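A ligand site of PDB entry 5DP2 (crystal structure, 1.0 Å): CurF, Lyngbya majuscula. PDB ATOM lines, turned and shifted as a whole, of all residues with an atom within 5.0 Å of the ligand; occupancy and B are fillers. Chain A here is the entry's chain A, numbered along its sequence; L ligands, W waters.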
ATOM      1  N   ASN A  49     -17.338   1.049  31.229  1.00  0.00           N
ATOM      2  CA  ASN A  49     -16.332   0.011  31.122  1.00  0.00           C
ATOM      3  C   ASN A  49     -16.985  -1.288  30.635  1.00  0.00           C
ATOM      4  O   ASN A  49     -18.157  -1.541  30.911  1.00  0.00           O
ATOM      5  CB  ASN A  49     -15.597  -0.187  32.456  1.00  0.00           C
ATOM      6  CG  ASN A  49     -14.523   0.911  32.658  1.00  0.00           C
ATOM      7  OD1 ASN A  49     -13.347   0.761  32.267  1.00  0.00           O
ATOM      8  ND2 ASN A  49     -14.923   2.030  33.163  1.00  0.00           N
ATOM      9  N   PHE A  50     -16.245  -2.132  29.941  1.00  0.00           N
ATOM     10  CA  PHE A  50     -16.814  -3.334  29.381  1.00  0.00           C
ATOM     11  C   PHE A  50     -17.402  -4.243  30.475  1.00  0.00           C
ATOM     12  O   PHE A  50     -18.463  -4.848  30.262  1.00  0.00           O
ATOM     13  CB  PHE A  50     -15.784  -4.093  28.542  1.00  0.00           C
ATOM     14  CG  PHE A  50     -16.365  -5.169  27.699  1.00  0.00           C
ATOM     15  CD1 PHE A  50     -17.173  -4.851  26.598  1.00  0.00           C
ATOM     16  CD2 PHE A  50     -16.116  -6.488  27.996  1.00  0.00           C
ATOM     17  CE1 PHE A  50     -17.709  -5.855  25.802  1.00  0.00           C
ATOM     18  CE2 PHE A  50     -16.634  -7.502  27.194  1.00  0.00           C
ATOM     19  CZ  PHE A  50     -17.434  -7.180  26.094  1.00  0.00           C
ATOM     20  N   ARG A  51     -16.739  -4.365  31.639  1.00  0.00           N
ATOM     21  CA  ARG A  51     -17.297  -5.134  32.776  1.00  0.00           C
ATOM     22  C   ARG A  51     -18.724  -4.757  33.055  1.00  0.00           C
ATOM     23  O   ARG A  51     -19.547  -5.607  33.421  1.00  0.00           O
ATOM     24  CB  ARG A  51     -16.447  -4.894  34.084  1.00  0.00           C
ATOM     25  CG  ARG A  51     -17.032  -5.519  35.375  1.00  0.00           C
ATOM     26  CD  ARG A  51     -16.984  -7.023  35.416  1.00  0.00           C
ATOM     27  NE  ARG A  51     -15.637  -7.505  35.617  1.00  0.00           N
ATOM     28  CZ  ARG A  51     -14.986  -7.652  36.794  1.00  0.00           C
ATOM     29  NH1 ARG A  51     -15.567  -7.352  37.965  1.00  0.00           N
ATOM     30  NH2 ARG A  51     -13.750  -8.101  36.777  1.00  0.00           N
ATOM     31  N   LEU A  54     -21.162  -6.305  30.759  1.00  0.00           N
ATOM     32  CA  LEU A  54     -21.332  -7.697  31.157  1.00  0.00           C
ATOM     33  C   LEU A  54     -22.192  -7.790  32.414  1.00  0.00           C
ATOM     34  O   LEU A  54     -22.990  -8.721  32.564  1.00  0.00           O
ATOM     35  CB  LEU A  54     -19.972  -8.377  31.397  1.00  0.00           C
ATOM     36  CG  LEU A  54     -18.981  -8.420  30.241  1.00  0.00           C
ATOM     37  CD1 LEU A  54     -17.717  -9.137  30.687  1.00  0.00           C
ATOM     38  CD2 LEU A  54     -19.602  -9.065  29.009  1.00  0.00           C
ATOM     39  N   MET A 141      -9.088   3.634  34.739  1.00  0.00           N
ATOM     40  CA  MET A 141      -9.096   2.188  34.709  1.00  0.00           C
ATOM     41  C   MET A 141      -8.185   1.664  33.582  1.00  0.00           C
ATOM     42  O   MET A 141      -7.443   0.690  33.784  1.00  0.00           O
ATOM     43  CB  MET A 141     -10.512   1.664  34.600  1.00  0.00           C
ATOM     44  CG  MET A 141     -10.625   0.177  34.775  1.00  0.00           C
ATOM     45  SD  MET A 141     -10.080  -0.525  36.320  1.00  0.00           S
ATOM     46  CE  MET A 141     -11.491  -0.158  37.358  1.00  0.00           C
ATOM     47  N   SER A 142      -8.246   2.264  32.412  1.00  0.00           N
ATOM     48  CA  SER A 142      -7.501   1.728  31.269  1.00  0.00           C
ATOM     49  C   SER A 142      -5.976   1.848  31.481  1.00  0.00           C
ATOM     50  O   SER A 142      -5.247   0.880  31.266  1.00  0.00           O
ATOM     51  CB  SER A 142      -7.942   2.377  29.977  1.00  0.00           C
ATOM     52  OG  SER A 142      -9.307   2.157  29.705  1.00  0.00           O
ATOM     53  N   THR A 145      -4.691  -0.266  34.637  1.00  0.00           N
ATOM     54  CA  THR A 145      -4.622  -1.691  34.289  1.00  0.00           C
ATOM     55  C   THR A 145      -3.418  -1.966  33.406  1.00  0.00           C
ATOM     56  O   THR A 145      -2.638  -2.897  33.654  1.00  0.00           O
ATOM     57  CB  THR A 145      -5.927  -2.084  33.569  1.00  0.00           C
ATOM     58  OG1 THR A 145      -7.043  -1.900  34.444  1.00  0.00           O
ATOM     59  CG2 THR A 145      -5.920  -3.538  33.137  1.00  0.00           C
ATOM     60  N   ALA A 166      -7.106  -6.678  20.993  1.00  0.00           N
ATOM     61  CA  ALA A 166      -8.204  -5.720  21.149  1.00  0.00           C
ATOM     62  C   ALA A 166      -7.618  -4.323  21.365  1.00  0.00           C
ATOM     63  O   ALA A 166      -8.048  -3.543  22.233  1.00  0.00           O
ATOM     64  CB  ALA A 166      -9.172  -6.108  22.253  1.00  0.00           C
ATOM     65  N   SER A 168      -7.879  -1.625  19.804  1.00  0.00           N
ATOM     66  CA  SER A 168      -8.819  -0.542  19.581  1.00  0.00           C
ATOM     67  C   SER A 168      -9.597  -0.124  20.831  1.00  0.00           C
ATOM     68  O   SER A 168     -10.183   0.949  20.810  1.00  0.00           O
ATOM     69  CB  SER A 168      -9.806  -1.067  18.524  1.00  0.00           C
ATOM     70  OG  SER A 168     -10.091  -2.472  18.751  1.00  0.00           O
ATOM     71  N   GLY A 169      -9.664  -1.001  21.834  1.00  0.00           N
ATOM     72  CA  GLY A 169     -10.471  -0.732  23.005  1.00  0.00           C
ATOM     73  C   GLY A 169      -9.746   0.114  24.041  1.00  0.00           C
ATOM     74  O   GLY A 169      -8.664   0.639  23.792  1.00  0.00           O
ATOM     75  N   GLY A 170     -10.362   0.296  25.200  1.00  0.00           N
ATOM     76  CA  GLY A 170      -9.811   1.191  26.211  1.00  0.00           C
ATOM     77  C   GLY A 170      -8.491   0.685  26.781  1.00  0.00           C
ATOM     78  O   GLY A 170      -7.455   1.375  26.727  1.00  0.00           O
ATOM     79  N   ALA A 171      -8.525  -0.524  27.340  1.00  0.00           N
ATOM     80  CA  ALA A 171      -7.302  -1.096  27.888  1.00  0.00           C
ATOM     81  C   ALA A 171      -6.240  -1.228  26.811  1.00  0.00           C
ATOM     82  O   ALA A 171      -5.055  -0.965  27.034  1.00  0.00           O
ATOM     83  CB  ALA A 171      -7.597  -2.433  28.562  1.00  0.00           C
ATOM     84  N   THR A 190      -7.018  -6.231  16.118  1.00  0.00           N
ATOM     85  CA  THR A 190      -8.304  -5.558  16.215  1.00  0.00           C
ATOM     86  C   THR A 190      -9.211  -6.127  15.115  1.00  0.00           C
ATOM     87  O   THR A 190      -8.786  -6.899  14.251  1.00  0.00           O
ATOM     88  CB  THR A 190      -8.149  -4.020  16.102  1.00  0.00           C
ATOM     89  OG1 THR A 190      -9.387  -3.397  16.359  1.00  0.00           O
ATOM     90  CG2 THR A 190      -7.676  -3.583  14.731  1.00  0.00           C
ATOM     91  N   SER A 191     -10.474  -5.738  15.142  1.00  0.00           N
ATOM     92  CA  SER A 191     -11.425  -6.244  14.155  1.00  0.00           C
ATOM     93  C   SER A 191     -11.089  -5.664  12.773  1.00  0.00           C
ATOM     94  O   SER A 191     -10.521  -4.566  12.657  1.00  0.00           O
ATOM     95  CB  SER A 191     -12.826  -5.870  14.571  1.00  0.00           C
ATOM     96  OG  SER A 191     -13.185  -6.487  15.800  1.00  0.00           O
ATOM     97  N   LYS A 194     -11.363  -1.916  11.872  1.00  0.00           N
ATOM     98  CA  LYS A 194     -10.566  -1.012  12.701  1.00  0.00           C
ATOM     99  C   LYS A 194      -9.075  -1.089  12.408  1.00  0.00           C
ATOM    100  O   LYS A 194      -8.318  -0.264  12.918  1.00  0.00           O
ATOM    101  CB  LYS A 194     -10.838  -1.266  14.187  1.00  0.00           C
ATOM    102  CG  LYS A 194     -12.296  -1.133  14.576  1.00  0.00           C
ATOM    103  CD  LYS A 194     -12.516  -1.296  16.073  1.00  0.00           C
ATOM    104  CE  LYS A 194     -13.994  -1.362  16.427  1.00  0.00           C
ATOM    105  NZ  LYS A 194     -14.216  -1.354  17.906  1.00  0.00           N
ATOM    106  N   SER A 209      -8.089  -9.696  14.954  1.00  0.00           N
ATOM    107  CA  SER A 209      -8.296 -10.347  16.226  1.00  0.00           C
ATOM    108  C   SER A 209      -9.444 -11.346  16.271  1.00  0.00           C
ATOM    109  O   SER A 209      -9.593 -12.054  17.259  1.00  0.00           O
ATOM    110  CB  SER A 209      -8.660  -9.304  17.258  1.00  0.00           C
ATOM    111  OG  SER A 209      -9.867  -8.672  16.829  1.00  0.00           O
ATOM    112  N   ARG A 210     -10.281 -11.361  15.223  1.00  0.00           N
ATOM    113  CA  ARG A 210     -11.564 -12.043  15.271  1.00  0.00           C
ATOM    114  C   ARG A 210     -11.477 -13.519  14.923  1.00  0.00           C
ATOM    115  O   ARG A 210     -12.482 -14.237  15.029  1.00  0.00           O
ATOM    116  CB  ARG A 210     -12.599 -11.334  14.390  1.00  0.00           C
ATOM    117  CG  ARG A 210     -12.999  -9.983  14.943  1.00  0.00           C
ATOM    118  CD  ARG A 210     -14.157 -10.118  15.909  1.00  0.00           C
ATOM    119  NE  ARG A 210     -14.393  -8.864  16.641  1.00  0.00           N
ATOM    120  CZ  ARG A 210     -15.339  -8.708  17.571  1.00  0.00           C
ATOM    121  NH1 ARG A 210     -16.174  -9.694  17.852  1.00  0.00           N
ATOM    122  NH2 ARG A 210     -15.478  -7.556  18.214  1.00  0.00           N
ATOM    123  N   SER A 233      -7.053  -9.971  26.645  1.00  0.00           N
ATOM    124  CA  SER A 233      -8.365 -10.020  27.267  1.00  0.00           C
ATOM    125  C   SER A 233      -9.322 -11.014  26.583  1.00  0.00           C
ATOM    126  O   SER A 233     -10.468 -11.111  27.005  1.00  0.00           O
ATOM    127  CB  SER A 233      -9.002  -8.647  27.292  1.00  0.00           C
ATOM    128  OG  SER A 233      -9.262  -8.168  25.988  1.00  0.00           O
ATOM    129  N   LEU A 234      -8.891 -11.696  25.517  1.00  0.00           N
ATOM    130  CA  LEU A 234      -9.784 -12.569  24.738  1.00  0.00           C
ATOM    131  C   LEU A 234      -9.581 -14.000  25.197  1.00  0.00           C
ATOM    132  O   LEU A 234      -8.520 -14.591  24.983  1.00  0.00           O
ATOM    133  CB  LEU A 234      -9.477 -12.415  23.243  1.00  0.00           C
ATOM    134  CG  LEU A 234      -9.538 -10.980  22.692  1.00  0.00           C
ATOM    135  CD1 LEU A 234      -9.198 -10.950  21.212  1.00  0.00           C
ATOM    136  CD2 LEU A 234     -10.894 -10.335  22.954  1.00  0.00           C
ATOM    137  N   HIS A 236     -12.147 -16.693  25.029  1.00  0.00           N
ATOM    138  CA  HIS A 236     -13.060 -17.706  24.487  1.00  0.00           C
ATOM    139  C   HIS A 236     -12.325 -18.613  23.488  1.00  0.00           C
ATOM    140  O   HIS A 236     -11.184 -18.352  23.088  1.00  0.00           O
ATOM    141  CB  HIS A 236     -14.255 -17.008  23.835  1.00  0.00           C
ATOM    142  CG  HIS A 236     -13.870 -16.088  22.735  1.00  0.00           C
ATOM    143  ND1 HIS A 236     -13.297 -14.856  22.962  1.00  0.00           N
ATOM    144  CD2 HIS A 236     -13.935 -16.226  21.393  1.00  0.00           C
ATOM    145  CE1 HIS A 236     -13.052 -14.270  21.813  1.00  0.00           C
ATOM    146  NE2 HIS A 236     -13.425 -15.078  20.838  1.00  0.00           N
ATOM    147  N   TYR A 239      -8.371 -19.098  22.063  1.00  0.00           N
ATOM    148  CA  TYR A 239      -7.502 -17.940  22.171  1.00  0.00           C
ATOM    149  C   TYR A 239      -6.407 -18.112  23.217  1.00  0.00           C
ATOM    150  O   TYR A 239      -5.273 -17.681  22.970  1.00  0.00           O
ATOM    151  CB  TYR A 239      -8.324 -16.662  22.437  1.00  0.00           C
ATOM    152  CG  TYR A 239      -8.934 -16.072  21.174  1.00  0.00           C
ATOM    153  CD1 TYR A 239     -10.046 -16.650  20.555  1.00  0.00           C
ATOM    154  CD2 TYR A 239      -8.380 -14.964  20.569  1.00  0.00           C
ATOM    155  CE1 TYR A 239     -10.555 -16.125  19.390  1.00  0.00           C
ATOM    156  CE2 TYR A 239      -8.890 -14.418  19.412  1.00  0.00           C
ATOM    157  CZ  TYR A 239      -9.974 -15.009  18.808  1.00  0.00           C
ATOM    158  OH  TYR A 239     -10.529 -14.512  17.667  1.00  0.00           O
ATOM    159  N   ILE A 256      -6.019 -10.167  31.408  1.00  0.00           N
ATOM    160  CA  ILE A 256      -6.988  -9.331  32.101  1.00  0.00           C
ATOM    161  C   ILE A 256      -8.421  -9.792  31.878  1.00  0.00           C
ATOM    162  O   ILE A 256      -9.328  -9.272  32.519  1.00  0.00           O
ATOM    163  CB  ILE A 256      -6.817  -7.824  31.791  1.00  0.00           C
ATOM    164  CG1 ILE A 256      -7.223  -7.458  30.354  1.00  0.00           C
ATOM    165  CG2 ILE A 256      -5.384  -7.388  32.101  1.00  0.00           C
ATOM    166  CD1 ILE A 256      -7.234  -5.966  30.069  1.00  0.00           C
ATOM    167  N   GLY A 257      -8.663 -10.753  30.986  1.00  0.00           N
ATOM    168  CA  GLY A 257      -9.989 -11.326  30.918  1.00  0.00           C
ATOM    169  C   GLY A 257     -10.246 -12.116  32.203  1.00  0.00           C
ATOM    170  O   GLY A 257      -9.303 -12.607  32.820  1.00  0.00           O
ATOM    171  N   ARG A 258     -11.503 -12.178  32.612  1.00  0.00           N
ATOM    172  CA  ARG A 258     -11.817 -12.894  33.843  1.00  0.00           C
ATOM    173  C   ARG A 258     -12.730 -14.081  33.618  1.00  0.00           C
ATOM    174  O   ARG A 258     -12.962 -14.831  34.552  1.00  0.00           O
ATOM    175  CB  ARG A 258     -12.335 -11.923  34.930  1.00  0.00           C
ATOM    176  CG  ARG A 258     -11.365 -10.791  35.280  1.00  0.00           C
ATOM    177  CD  ARG A 258     -10.050 -11.285  35.843  1.00  0.00           C
ATOM    178  NE  ARG A 258     -10.216 -11.932  37.136  1.00  0.00           N
ATOM    179  CZ  ARG A 258      -9.254 -12.520  37.832  1.00  0.00           C
ATOM    180  NH1 ARG A 258      -8.030 -12.675  37.318  1.00  0.00           N
ATOM    181  NH2 ARG A 258      -9.526 -12.996  39.037  1.00  0.00           N
ATOM    182  N   PHE A 279      -4.772 -10.987  36.591  1.00  0.00           N
ATOM    183  CA  PHE A 279      -5.097 -10.121  37.713  1.00  0.00           C
ATOM    184  C   PHE A 279      -6.429  -9.451  37.478  1.00  0.00           C
ATOM    185  O   PHE A 279      -6.916  -9.378  36.339  1.00  0.00           O
ATOM    186  CB  PHE A 279      -4.005  -9.060  37.997  1.00  0.00           C
ATOM    187  CG  PHE A 279      -3.766  -8.079  36.863  1.00  0.00           C
ATOM    188  CD1 PHE A 279      -2.874  -8.359  35.845  1.00  0.00           C
ATOM    189  CD2 PHE A 279      -4.409  -6.861  36.828  1.00  0.00           C
ATOM    190  CE1 PHE A 279      -2.641  -7.427  34.843  1.00  0.00           C
ATOM    191  CE2 PHE A 279      -4.184  -5.951  35.807  1.00  0.00           C
ATOM    192  CZ  PHE A 279      -3.282  -6.232  34.809  1.00  0.00           C
ATOM    193  N   ASP A 280      -7.005  -8.907  38.562  1.00  0.00           N
ATOM    194  CA  ASP A 280      -8.255  -8.159  38.536  1.00  0.00           C
ATOM    195  C   ASP A 280      -8.038  -6.879  39.328  1.00  0.00           C
ATOM    196  O   ASP A 280      -7.830  -6.919  40.560  1.00  0.00           O
ATOM    197  CB  ASP A 280      -9.421  -8.990  39.078  1.00  0.00           C
ATOM    198  CG  ASP A 280     -10.768  -8.280  38.935  1.00  0.00           C
ATOM    199  OD1 ASP A 280     -10.785  -7.055  39.030  1.00  0.00           O
ATOM    200  OD2 ASP A 280     -11.807  -8.948  38.728  1.00  0.00           O
ATOM    201  N   MET A 281      -8.022  -5.756  38.618  1.00  0.00           N
ATOM    202  CA  MET A 281      -7.744  -4.485  39.285  1.00  0.00           C
ATOM    203  C   MET A 281      -8.735  -4.134  40.370  1.00  0.00           C
ATOM    204  O   MET A 281      -8.358  -3.524  41.374  1.00  0.00           O
ATOM    205  CB  MET A 281      -7.699  -3.361  38.262  1.00  0.00           C
ATOM    206  CG  MET A 281      -6.556  -3.465  37.299  1.00  0.00           C
ATOM    207  SD  MET A 281      -4.907  -3.254  38.047  1.00  0.00           S
ATOM    208  CE  MET A 281      -4.889  -1.474  38.197  1.00  0.00           C
ATOM    209  N   SER A 282     -10.016  -4.482  40.173  1.00  0.00           N
ATOM    210  CA  SER A 282     -10.981  -4.228  41.228  1.00  0.00           C
ATOM    211  C   SER A 282     -10.599  -4.925  42.547  1.00  0.00           C
ATOM    212  O   SER A 282     -10.660  -4.326  43.625  1.00  0.00           O
ATOM    213  CB  SER A 282     -12.404  -4.551  40.758  1.00  0.00           C
ATOM    214  OG  SER A 282     -12.600  -5.901  40.485  1.00  0.00           O
ATOM    215  N   LEU A 328     -20.640   0.556  23.304  1.00  0.00           N
ATOM    216  CA  LEU A 328     -19.575  -0.342  23.755  1.00  0.00           C
ATOM    217  C   LEU A 328     -19.940  -1.811  23.509  1.00  0.00           C
ATOM    218  O   LEU A 328     -19.118  -2.570  23.005  1.00  0.00           O
ATOM    219  CB  LEU A 328     -19.250  -0.073  25.242  1.00  0.00           C
ATOM    220  CG  LEU A 328     -18.048  -0.824  25.764  1.00  0.00           C
ATOM    221  CD1 LEU A 328     -16.798  -0.680  24.915  1.00  0.00           C
ATOM    222  CD2 LEU A 328     -17.802  -0.421  27.201  1.00  0.00           C
ATOM    223  N   SER A 331     -19.407  -2.571  20.062  1.00  0.00           N
ATOM    224  CA  SER A 331     -18.014  -2.333  19.768  1.00  0.00           C
ATOM    225  C   SER A 331     -17.813  -1.386  18.624  1.00  0.00           C
ATOM    226  O   SER A 331     -17.072  -1.666  17.678  1.00  0.00           O
ATOM    227  CB  SER A 331     -17.293  -3.640  19.506  1.00  0.00           C
ATOM    228  OG  SER A 331     -15.963  -3.459  19.904  1.00  0.00           O
ATOM    229  N   HIS A 333     -16.505   1.539  18.778  1.00  0.00           N
ATOM    230  CA  HIS A 333     -15.600   2.574  19.287  1.00  0.00           C
ATOM    231  C   HIS A 333     -14.122   2.336  18.996  1.00  0.00           C
ATOM    232  O   HIS A 333     -13.667   1.246  18.683  1.00  0.00           O
ATOM    233  CB  HIS A 333     -15.784   2.625  20.812  1.00  0.00           C
ATOM    234  CG  HIS A 333     -15.328   1.380  21.482  1.00  0.00           C
ATOM    235  ND1 HIS A 333     -15.768   0.124  21.098  1.00  0.00           N
ATOM    236  CD2 HIS A 333     -14.426   1.197  22.470  1.00  0.00           C
ATOM    237  CE1 HIS A 333     -15.129  -0.769  21.842  1.00  0.00           C
ATOM    238  NE2 HIS A 333     -14.325  -0.146  22.690  1.00  0.00           N
ATOM    239  N   GLY A 335     -11.052   3.516  21.684  1.00  0.00           N
ATOM    240  CA  GLY A 335     -10.759   4.219  22.934  1.00  0.00           C
ATOM    241  C   GLY A 335     -11.878   4.098  23.958  1.00  0.00           C
ATOM    242  O   GLY A 335     -12.258   2.962  24.327  1.00  0.00           O
HETATM  243  P1  LIG L   1     -12.820  -2.416  25.417  1.00  0.00           P
HETATM  244  O1  LIG L   1     -12.972  -0.981  25.054  1.00  0.00           O
HETATM  245  O2  LIG L   1     -11.515  -3.089  25.201  1.00  0.00           O
HETATM  246  O3  LIG L   1     -13.997  -3.214  24.683  1.00  0.00           O
HETATM  247  C1  LIG L   1     -13.951  -4.639  24.539  1.00  0.00           C
HETATM  248  C2  LIG L   1     -12.981  -5.102  23.477  1.00  0.00           C
HETATM  249  O4  LIG L   1     -13.150  -6.483  23.288  1.00  0.00           O
HETATM  250  C3  LIG L   1     -13.164  -4.425  22.150  1.00  0.00           C
HETATM  251  O5  LIG L   1     -11.986  -3.672  21.866  1.00  0.00           O
HETATM  252  C4  LIG L   1     -13.366  -5.562  21.133  1.00  0.00           C
HETATM  253  O6  LIG L   1     -12.612  -5.532  19.953  1.00  0.00           O
HETATM  254  C5  LIG L   1     -12.892  -6.787  21.906  1.00  0.00           C
HETATM  255  N1  LIG L   1     -13.652  -8.001  21.620  1.00  0.00           N
HETATM  256  C6  LIG L   1     -14.827  -8.404  22.213  1.00  0.00           C
HETATM  257  N2  LIG L   1     -15.225  -9.593  21.703  1.00  0.00           N
HETATM  258  C7  LIG L   1     -14.305  -9.959  20.810  1.00  0.00           C
HETATM  259  C8  LIG L   1     -14.124 -11.076  19.942  1.00  0.00           C
HETATM  260  N3  LIG L   1     -15.031 -12.077  19.941  1.00  0.00           N
HETATM  261  N4  LIG L   1     -13.051 -11.112  19.160  1.00  0.00           N
HETATM  262  C9  LIG L   1     -12.175 -10.105  19.186  1.00  0.00           C
HETATM  263  N5  LIG L   1     -12.235  -9.006  19.955  1.00  0.00           N
HETATM  264  C10 LIG L   1     -13.294  -8.936  20.739  1.00  0.00           C
HETATM  265  O7  LIG L   1     -13.242  -2.627  26.960  1.00  0.00           O
HETATM  266  P2  LIG L   1     -12.416  -2.314  28.298  1.00  0.00           P
HETATM  267  O8  LIG L   1     -13.380  -1.779  29.291  1.00  0.00           O
HETATM  268  O9  LIG L   1     -11.188  -1.516  27.986  1.00  0.00           O
HETATM  269  O10 LIG L   1     -12.032  -3.757  28.764  1.00  0.00           O
HETATM  270  C11 LIG L   1     -11.100  -4.516  27.953  1.00  0.00           C
HETATM  271  C12 LIG L   1     -11.166  -6.010  28.359  1.00  0.00           C
HETATM  272  O11 LIG L   1     -10.397  -6.176  29.522  1.00  0.00           O
HETATM  273  C13 LIG L   1     -12.565  -6.524  28.727  1.00  0.00           C
HETATM  274  O12 LIG L   1     -12.613  -7.926  28.447  1.00  0.00           O
HETATM  275  C14 LIG L   1     -12.654  -6.238  30.200  1.00  0.00           C
HETATM  276  O13 LIG L   1     -13.591  -7.111  30.832  1.00  0.00           O
HETATM  277  C15 LIG L   1     -11.233  -6.474  30.644  1.00  0.00           C
HETATM  278  N6  LIG L   1     -10.655  -5.678  31.754  1.00  0.00           N
HETATM  279  C16 LIG L   1     -10.085  -6.318  32.806  1.00  0.00           C
HETATM  280  C17 LIG L   1      -9.513  -5.620  33.867  1.00  0.00           C
HETATM  281  C18 LIG L   1      -8.905  -6.371  35.002  1.00  0.00           C
HETATM  282  O14 LIG L   1      -8.615  -5.701  35.971  1.00  0.00           O
HETATM  283  N7  LIG L   1      -8.712  -7.713  34.884  1.00  0.00           N
HETATM  284  C19 LIG L   1      -9.510  -4.230  33.843  1.00  0.00           C
HETATM  285  C20 LIG L   1     -10.094  -3.594  32.748  1.00  0.00           C
HETATM  286  C21 LIG L   1     -10.658  -4.332  31.702  1.00  0.00           C
HETATM  287  P3  LIG L   1     -12.911  -4.574  18.711  1.00  0.00           P
HETATM  288  O15 LIG L   1     -12.600  -3.161  19.185  1.00  0.00           O
HETATM  289  O16 LIG L   1     -11.955  -5.082  17.674  1.00  0.00           O
HETATM  290  O17 LIG L   1     -14.366  -4.755  18.362  1.00  0.00           O
HETATM  291  O   HOH W   1     -15.359 -14.231  17.541  1.00  0.00           O
HETATM  292  O   HOH W   2     -13.056 -13.773  18.340  1.00  0.00           O
HETATM  293  O   HOH W   3      -8.857  -3.418  24.918  1.00  0.00           O
HETATM  294  O   HOH W   4     -12.277  -1.452  31.695  1.00  0.00           O
HETATM  295  O   HOH W   5     -17.461 -10.481  23.722  1.00  0.00           O
HETATM  296  O   HOH W   6     -17.614 -12.258  21.354  1.00  0.00           O
HETATM  297  O   HOH W   7     -14.299 -10.176  29.278  1.00  0.00           O
HETATM  298  O   HOH W   8     -13.229   1.032  29.032  1.00  0.00           O
HETATM  299  O   HOH W   9     -10.320  -7.032  18.842  1.00  0.00           O
HETATM  300  O   HOH W  10     -13.528   1.397  26.223  1.00  0.00           O
HETATM  301  O   HOH W  11     -13.601 -10.333  31.642  1.00  0.00           O
HETATM  302  O   HOH W  12     -11.651  -4.989  37.124  1.00  0.00           O
HETATM  303  O   HOH W  13     -10.029  -0.411  30.251  1.00  0.00           O
HETATM  304  O   HOH W  14     -17.294  -6.653  22.561  1.00  0.00           O
HETATM  305  O   HOH W  15     -13.236  -7.826  33.598  1.00  0.00           O
HETATM  306  O   HOH W  16     -12.056  -7.983  25.576  1.00  0.00           O
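O of Phe 279 is in hydrogen-bond range of N7 of the ligand, at 2.8 Å. A ring nitrogen (NE2) of His 333 lies within hydrogen-bond range of an oxygen (O1) of the ligand, at 2.8 Å. O16 of the ligand sits at hydrogen-bond distance from OG of Ser 191, 2.6 Å away. An oxygen (O17) of the ligand lies within salt-bridge range of the guanidinium group (NH2) of Arg 210. An oxygen (O15) of the ligand is in hydrogen-bond range of the side-chain hydroxyl (OG) of Ser 168 (2.6 Å). The backbone NH of Ala 171 lies within hydrogen-bond range of an oxygen (O9) of the ligand (2.9 Å). The backbone NH (N) of Gly 170 lies within hydrogen-bond range of an oxygen (O1) of the ligand, at 2.9 Å. The side-chain hydroxyl (OG1) of Thr 190 sits at hydrogen-bond distance from an oxygen (O16) of the ligand. The side-chain hydroxyl of Ser 331 sits at hydrogen-bond distance from an oxygen (O17) of the ligand (2.6 Å). The side-chain amino group (NZ) of Lys 194 lies within salt-bridge range of an oxygen (O15) of the ligand (2.7 Å). An oxygen (O8) of the ligand is in hydrogen-bond range of the backbone NH (N) of Phe 50 (3.0 Å). The backbone carbonyl oxygen of Ile 256 sits at hydrogen-bond distance from a nitrogen (N7) of the ligand (2.9 Å). The backbone NH of Ser 191 sits at hydrogen-bond distance from an oxygen (O16) of the ligand, 3.0 Å away. N of Met 281 sits at hydrogen-bond distance from O14 of the ligand, at 2.7 Å.
N of Ser 191 sits at hydrogen-bond distance from OG of Ser 209, at 3.4 Å. The side-chain hydroxyl (OH) of Tyr 239 sits close to the backbone carbonyl oxygen (O) of Arg 210. The backbone carbonyl oxygen of Ser 331 is in hydrogen-bond range of the side-chain amino group of Lys 194 (2.9 Å). The side-chain carboxylate (OD2) of Asp 280 lies within salt-bridge range of the guanidinium group (NE) of Arg 258. O of Met 141 is in hydrogen-bond range of OG1 of Thr 145. O of Ser 168 sits at hydrogen-bond distance from N of Gly 335, 2.8 Å away. The side-chain carboxylate (OD1) of Asp 280 lies within hydrogen-bond range of the side-chain hydroxyl (OG) of Ser 282 (2.6 Å). The backbone NH (N) of Ser 209 is in hydrogen-bond range of the backbone carbonyl oxygen (O) of Thr 190 (3.0 Å).
Merely in contact with the ligand: Asn 49 (3.9 Å), Thr 145 (3.4 Å), Ala 166 (3.7 Å), Gly 169 (3.2 Å), Ser 209 (3.6 Å), Ser 233 (3.6 Å), Leu 234 (3.5 Å), His 236 (3.5 Å), Arg 258 (3.9 Å), Asp 280 (3.6 Å) and Leu 328 (3.8 Å). Hydrophobic or aromatic side chains within 4 Å of the ligand: Phe 50, Ala 166, Ala 171, Leu 234, His 236, Ile 256, Met 281, Leu 328 and His 333. Within 4 Å of the ligand: Asn 49, Phe 50, Thr 145, Ala 166, Ser 168, Gly 169, Gly 170, Ala 171, Thr 190, Ser 191, Lys 194, Ser 209, Arg 210, Ser 233, Leu 234, His 236, Ile 256, Arg 258, Phe 279, Asp 280, Met 281, Leu 328, Ser 331 and His 333. Along chain A the residues within 4 Å of the ligand span positions 49 to 333. The nearest printed residue that does not touch the ligand is Gly 335 (4.1 Å).
Water W13 lies within hydrogen-bond range of the side-chain hydroxyl of Ser 142, an oxygen (O9) of the ligand and the backbone NH of Ala 171. Water W2 lies within hydrogen-bond range of OH of Tyr 239 (2.7 Å), N4 of the ligand (2.8 Å), NE2 of His 236 (2.8 Å) and O of Arg 210 (3.4 Å). Water W9 bridges OG of Ser 209 (2.6 Å) and O16 of the ligand (2.8 Å). Water W15 lies within hydrogen-bond range of O13 of the ligand and NE of Arg 51. Water W16 lies within hydrogen-bond range of the side-chain hydroxyl of Ser 233 (2.8 Å) and an oxygen (O12) of the ligand (2.9 Å). Water W12 lies within hydrogen-bond range of OD1 of Asp 280 (2.9 Å), O14 of the ligand (3.3 Å) and N of Ser 282 (3.5 Å).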
